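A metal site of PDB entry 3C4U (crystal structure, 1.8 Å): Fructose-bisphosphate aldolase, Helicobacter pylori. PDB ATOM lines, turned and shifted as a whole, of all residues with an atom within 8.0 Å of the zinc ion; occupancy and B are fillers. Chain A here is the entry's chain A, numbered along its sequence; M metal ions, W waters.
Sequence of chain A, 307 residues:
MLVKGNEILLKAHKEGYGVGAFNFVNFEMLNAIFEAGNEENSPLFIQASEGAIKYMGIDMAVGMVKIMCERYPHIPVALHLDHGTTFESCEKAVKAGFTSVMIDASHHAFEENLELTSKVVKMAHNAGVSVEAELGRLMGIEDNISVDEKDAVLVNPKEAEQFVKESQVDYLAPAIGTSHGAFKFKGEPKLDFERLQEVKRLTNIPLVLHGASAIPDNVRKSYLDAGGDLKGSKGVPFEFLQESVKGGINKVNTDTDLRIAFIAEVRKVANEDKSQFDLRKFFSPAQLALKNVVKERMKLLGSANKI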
ATOM      1  N   ASP A  82     -32.628 -20.721  -8.307  1.00  0.00           N
ATOM      2  CA  ASP A  82     -32.304 -22.025  -7.737  1.00  0.00           C
ATOM      3  C   ASP A  82     -31.720 -22.971  -8.776  1.00  0.00           C
ATOM      4  O   ASP A  82     -32.378 -23.318  -9.749  1.00  0.00           O
ATOM      5  CB  ASP A  82     -33.550 -22.642  -7.103  1.00  0.00           C
ATOM      6  CG  ASP A  82     -33.256 -23.935  -6.373  1.00  0.00           C
ATOM      7  OD1 ASP A  82     -32.066 -24.256  -6.179  1.00  0.00           O
ATOM      8  OD2 ASP A  82     -34.217 -24.634  -5.998  1.00  0.00           O
ATOM      9  N   HIS A  83     -30.465 -23.376  -8.557  1.00  0.00           N
ATOM     10  CA  HIS A  83     -29.787 -24.323  -9.431  1.00  0.00           C
ATOM     11  C   HIS A  83     -29.774 -23.902 -10.905  1.00  0.00           C
ATOM     12  O   HIS A  83     -30.229 -24.649 -11.770  1.00  0.00           O
ATOM     13  CB  HIS A  83     -30.407 -25.719  -9.304  1.00  0.00           C
ATOM     14  CG  HIS A  83     -29.961 -26.456  -8.075  1.00  0.00           C
ATOM     15  ND1 HIS A  83     -30.492 -26.234  -6.825  1.00  0.00           N
ATOM     16  CD2 HIS A  83     -29.016 -27.420  -7.910  1.00  0.00           C
ATOM     17  CE1 HIS A  83     -29.908 -27.018  -5.947  1.00  0.00           C
ATOM     18  NE2 HIS A  83     -29.007 -27.759  -6.580  1.00  0.00           N
ATOM     19  N   MET A 102     -27.709 -18.803  -8.350  1.00  0.00           N
ATOM     20  CA  MET A 102     -26.818 -19.933  -8.139  1.00  0.00           C
ATOM     21  C   MET A 102     -26.454 -20.586  -9.461  1.00  0.00           C
ATOM     22  O   MET A 102     -27.317 -20.890 -10.274  1.00  0.00           O
ATOM     23  CB  MET A 102     -27.472 -20.985  -7.238  1.00  0.00           C
ATOM     24  CG  MET A 102     -26.524 -22.130  -6.896  1.00  0.00           C
ATOM     25  SD  MET A 102     -27.252 -23.765  -7.074  1.00  0.00           S
ATOM     26  CE  MET A 102     -25.845 -24.802  -6.703  1.00  0.00           C
ATOM     27  N   ASP A 104     -24.848 -23.945 -10.819  1.00  0.00           N
ATOM     28  CA  ASP A 104     -24.492 -25.294 -10.409  1.00  0.00           C
ATOM     29  C   ASP A 104     -23.650 -26.013 -11.461  1.00  0.00           C
ATOM     30  O   ASP A 104     -24.171 -26.503 -12.463  1.00  0.00           O
ATOM     31  CB  ASP A 104     -25.744 -26.117 -10.100  1.00  0.00           C
ATOM     32  CG  ASP A 104     -25.417 -27.512  -9.599  1.00  0.00           C
ATOM     33  OD1 ASP A 104     -24.243 -27.744  -9.211  1.00  0.00           O
ATOM     34  OD2 ASP A 104     -26.315 -28.373  -9.590  1.00  0.00           O
ATOM     35  N   SER A 106     -21.335 -28.319 -10.205  1.00  0.00           N
ATOM     36  CA  SER A 106     -20.704 -29.237  -9.260  1.00  0.00           C
ATOM     37  C   SER A 106     -20.485 -30.623  -9.869  1.00  0.00           C
ATOM     38  O   SER A 106     -19.776 -31.449  -9.292  1.00  0.00           O
ATOM     39  CB  SER A 106     -21.550 -29.351  -7.990  1.00  0.00           C
ATOM     40  OG  SER A 106     -22.824 -29.892  -8.258  1.00  0.00           O
ATOM     41  N   GLU A 132     -24.262 -17.932  -5.690  1.00  0.00           N
ATOM     42  CA  GLU A 132     -24.038 -19.178  -4.965  1.00  0.00           C
ATOM     43  C   GLU A 132     -23.475 -20.238  -5.904  1.00  0.00           C
ATOM     44  O   GLU A 132     -23.837 -20.300  -7.076  1.00  0.00           O
ATOM     45  CB  GLU A 132     -25.342 -19.682  -4.353  1.00  0.00           C
ATOM     46  CG  GLU A 132     -25.214 -21.046  -3.688  1.00  0.00           C
ATOM     47  CD  GLU A 132     -26.545 -21.602  -3.225  1.00  0.00           C
ATOM     48  OE1 GLU A 132     -27.450 -20.803  -2.904  1.00  0.00           O
ATOM     49  OE2 GLU A 132     -26.680 -22.848  -3.193  1.00  0.00           O
ATOM     50  N   ALA A 133     -22.579 -21.066  -5.374  1.00  0.00           N
ATOM     51  CA  ALA A 133     -22.011 -22.168  -6.142  1.00  0.00           C
ATOM     52  C   ALA A 133     -22.044 -23.452  -5.320  1.00  0.00           C
ATOM     53  O   ALA A 133     -22.391 -23.431  -4.137  1.00  0.00           O
ATOM     54  CB  ALA A 133     -20.582 -21.844  -6.554  1.00  0.00           C
ATOM     55  N   GLU A 134     -21.713 -24.572  -5.960  1.00  0.00           N
ATOM     56  CA  GLU A 134     -21.737 -25.857  -5.284  1.00  0.00           C
ATOM     57  C   GLU A 134     -20.454 -26.641  -5.545  1.00  0.00           C
ATOM     58  O   GLU A 134     -19.911 -26.587  -6.647  1.00  0.00           O
ATOM     59  CB  GLU A 134     -22.949 -26.674  -5.728  1.00  0.00           C
ATOM     60  CG  GLU A 134     -23.196 -27.925  -4.915  1.00  0.00           C
ATOM     61  CD  GLU A 134     -24.577 -28.477  -5.159  1.00  0.00           C
ATOM     62  OE1 GLU A 134     -25.324 -27.852  -5.941  1.00  0.00           O
ATOM     63  OE2 GLU A 134     -24.926 -29.532  -4.578  1.00  0.00           O
ATOM     64  N   LEU A 135     -19.954 -27.335  -4.539  1.00  0.00           N
ATOM     65  CA  LEU A 135     -18.685 -28.044  -4.666  1.00  0.00           C
ATOM     66  C   LEU A 135     -18.675 -29.347  -3.862  1.00  0.00           C
ATOM     67  O   LEU A 135     -19.141 -29.400  -2.725  1.00  0.00           O
ATOM     68  CB  LEU A 135     -17.535 -27.150  -4.224  1.00  0.00           C
ATOM     69  CG  LEU A 135     -16.137 -27.750  -4.387  1.00  0.00           C
ATOM     70  CD1 LEU A 135     -15.860 -28.010  -5.855  1.00  0.00           C
ATOM     71  CD2 LEU A 135     -15.084 -26.822  -3.793  1.00  0.00           C
ATOM     72  N   ALA A 173     -22.396 -24.079  -1.469  1.00  0.00           N
ATOM     73  CA  ALA A 173     -23.093 -25.276  -1.043  1.00  0.00           C
ATOM     74  C   ALA A 173     -22.140 -26.482  -1.095  1.00  0.00           C
ATOM     75  O   ALA A 173     -21.945 -27.064  -2.163  1.00  0.00           O
ATOM     76  CB  ALA A 173     -24.318 -25.516  -1.924  1.00  0.00           C
ATOM     77  N   THR A 178     -25.515 -35.056   2.591  1.00  0.00           N
ATOM     78  CA  THR A 178     -26.839 -35.257   1.987  1.00  0.00           C
ATOM     79  C   THR A 178     -26.745 -35.937   0.631  1.00  0.00           C
ATOM     80  O   THR A 178     -25.823 -35.664  -0.151  1.00  0.00           O
ATOM     81  CB  THR A 178     -27.609 -33.933   1.831  1.00  0.00           C
ATOM     82  OG1 THR A 178     -26.879 -33.053   0.971  1.00  0.00           O
ATOM     83  CG2 THR A 178     -27.802 -33.262   3.181  1.00  0.00           C
ATOM     84  N   HIS A 180     -27.710 -35.899  -2.840  1.00  0.00           N
ATOM     85  CA  HIS A 180     -28.231 -34.824  -3.660  1.00  0.00           C
ATOM     86  C   HIS A 180     -27.368 -34.512  -4.886  1.00  0.00           C
ATOM     87  O   HIS A 180     -26.135 -34.558  -4.812  1.00  0.00           O
ATOM     88  CB  HIS A 180     -28.404 -33.568  -2.815  1.00  0.00           C
ATOM     89  CG  HIS A 180     -28.583 -32.309  -3.608  1.00  0.00           C
ATOM     90  ND1 HIS A 180     -29.819 -31.817  -3.953  1.00  0.00           N
ATOM     91  CD2 HIS A 180     -27.671 -31.449  -4.132  1.00  0.00           C
ATOM     92  CE1 HIS A 180     -29.671 -30.712  -4.651  1.00  0.00           C
ATOM     93  NE2 HIS A 180     -28.378 -30.463  -4.773  1.00  0.00           N
ATOM     94  N   GLY A 181     -28.022 -34.193  -5.988  1.00  0.00           N
ATOM     95  CA  GLY A 181     -27.343 -33.768  -7.207  1.00  0.00           C
ATOM     96  C   GLY A 181     -26.295 -34.734  -7.719  1.00  0.00           C
ATOM     97  O   GLY A 181     -26.594 -35.883  -8.041  1.00  0.00           O
ATOM     98  N   ALA A 182     -25.058 -34.256  -7.777  1.00  0.00           N
ATOM     99  CA  ALA A 182     -23.942 -35.060  -8.277  1.00  0.00           C
ATOM    100  C   ALA A 182     -23.300 -35.846  -7.144  1.00  0.00           C
ATOM    101  O   ALA A 182     -22.250 -36.476  -7.336  1.00  0.00           O
ATOM    102  CB  ALA A 182     -22.913 -34.179  -8.963  1.00  0.00           C
ATOM    103  N   PHE A 183     -23.925 -35.823  -5.974  1.00  0.00           N
ATOM    104  CA  PHE A 183     -23.382 -36.510  -4.803  1.00  0.00           C
ATOM    105  C   PHE A 183     -24.412 -37.447  -4.176  1.00  0.00           C
ATOM    106  O   PHE A 183     -24.439 -37.623  -2.961  1.00  0.00           O
ATOM    107  CB  PHE A 183     -22.905 -35.497  -3.765  1.00  0.00           C
ATOM    108  CG  PHE A 183     -22.300 -34.257  -4.358  1.00  0.00           C
ATOM    109  CD1 PHE A 183     -22.953 -33.039  -4.240  1.00  0.00           C
ATOM    110  CD2 PHE A 183     -21.091 -34.315  -5.024  1.00  0.00           C
ATOM    111  CE1 PHE A 183     -22.391 -31.892  -4.784  1.00  0.00           C
ATOM    112  CE2 PHE A 183     -20.540 -33.177  -5.578  1.00  0.00           C
ATOM    113  CZ  PHE A 183     -21.185 -31.960  -5.448  1.00  0.00           C
ATOM    114  N   VAL A 208     -24.375 -23.142   2.330  1.00  0.00           N
ATOM    115  CA  VAL A 208     -25.712 -23.560   1.920  1.00  0.00           C
ATOM    116  C   VAL A 208     -25.881 -25.070   1.976  1.00  0.00           C
ATOM    117  O   VAL A 208     -24.981 -25.822   1.609  1.00  0.00           O
ATOM    118  CB  VAL A 208     -26.024 -23.065   0.488  1.00  0.00           C
ATOM    119  CG1 VAL A 208     -27.469 -23.366   0.131  1.00  0.00           C
ATOM    120  CG2 VAL A 208     -25.727 -21.582   0.370  1.00  0.00           C
ATOM    121  N   LEU A 209     -27.055 -25.512   2.428  1.00  0.00           N
ATOM    122  CA  LEU A 209     -27.352 -26.931   2.539  1.00  0.00           C
ATOM    123  C   LEU A 209     -28.401 -27.363   1.514  1.00  0.00           C
ATOM    124  O   LEU A 209     -29.498 -26.818   1.466  1.00  0.00           O
ATOM    125  CB  LEU A 209     -27.841 -27.267   3.950  1.00  0.00           C
ATOM    126  CG  LEU A 209     -28.152 -28.741   4.243  1.00  0.00           C
ATOM    127  CD1 LEU A 209     -26.925 -29.617   3.964  1.00  0.00           C
ATOM    128  CD2 LEU A 209     -28.626 -28.905   5.673  1.00  0.00           C
ATOM    129  N   HIS A 210     -28.036 -28.338   0.682  1.00  0.00           N
ATOM    130  CA  HIS A 210     -28.919 -28.846  -0.364  1.00  0.00           C
ATOM    131  C   HIS A 210     -29.380 -30.262  -0.053  1.00  0.00           C
ATOM    132  O   HIS A 210     -28.692 -31.012   0.646  1.00  0.00           O
ATOM    133  CB  HIS A 210     -28.204 -28.808  -1.712  1.00  0.00           C
ATOM    134  CG  HIS A 210     -27.986 -27.435  -2.248  1.00  0.00           C
ATOM    135  ND1 HIS A 210     -27.789 -27.174  -3.590  1.00  0.00           N
ATOM    136  CD2 HIS A 210     -27.938 -26.232  -1.631  1.00  0.00           C
ATOM    137  CE1 HIS A 210     -27.622 -25.883  -3.766  1.00  0.00           C
ATOM    138  NE2 HIS A 210     -27.711 -25.287  -2.596  1.00  0.00           N
ATOM    139  N   GLY A 211     -30.541 -30.637  -0.578  1.00  0.00           N
ATOM    140  CA  GLY A 211     -31.057 -31.988  -0.422  1.00  0.00           C
ATOM    141  C   GLY A 211     -31.327 -32.400   1.011  1.00  0.00           C
ATOM    142  O   GLY A 211     -31.224 -33.570   1.363  1.00  0.00           O
ATOM    143  N   ASN A 253     -32.064 -24.914   1.665  1.00  0.00           N
ATOM    144  CA  ASN A 253     -33.024 -25.076   0.583  1.00  0.00           C
ATOM    145  C   ASN A 253     -34.247 -25.860   1.025  1.00  0.00           C
ATOM    146  O   ASN A 253     -34.136 -26.983   1.514  1.00  0.00           O
ATOM    147  CB  ASN A 253     -32.376 -25.754  -0.623  1.00  0.00           C
ATOM    148  CG  ASN A 253     -31.362 -24.858  -1.316  1.00  0.00           C
ATOM    149  OD1 ASN A 253     -30.758 -23.986  -0.689  1.00  0.00           O
ATOM    150  ND2 ASN A 253     -31.178 -25.079  -2.602  1.00  0.00           N
HETATM  151 ZN    ZN M   1     -27.311 -28.659  -5.389  1.00  0.00          ZN
HETATM  152  O   HOH W   1     -26.909 -30.033  -7.412  1.00  0.00           O
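Water W1 lies within hydrogen-bond range of the side-chain carboxylate (OD2) of Asp 104 (2.8 Å) and the side-chain carboxylate (OE2) of Glu 134 (3.5 Å).
The backbone NH of His 83 lies close to the side-chain sulfur of Met 102 (3.6 Å). The backbone carbonyl oxygen of His 210 is in hydrogen-bond range of the side-chain hydroxyl of Thr 178, 2.7 Å away. ND1 of His 83 is in hydrogen-bond range of OD1 of Asp 82, at 2.6 Å. A ring nitrogen (NE2) of His 210 is in hydrogen-bond range of the side-chain amide nitrogen (ND2) of Asn 253 (3.5 Å). OE2 of Glu 132 lies within hydrogen-bond range of NE2 of His 210.
NE2 of His 180 binds the zinc ion (2.2 Å). The zinc ion is bound by OE1 of Glu 134 (2.2 Å). NE2 of His 83 is bound to the zinc ion (2.3 Å). ND1 of His 210 binds the zinc ion (2.4 Å). The zinc ion is bound by water W1 (2.5 Å). Slightly farther from the zinc ion lies the side-chain carboxylate (OE2) of Glu 134 (2.7 Å).
Within 4 Å of the zinc ion: His 83, Glu 134, His 180 and His 210. The nearest printed residue that does not touch the zinc ion is Asp 104 (4.3 Å).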
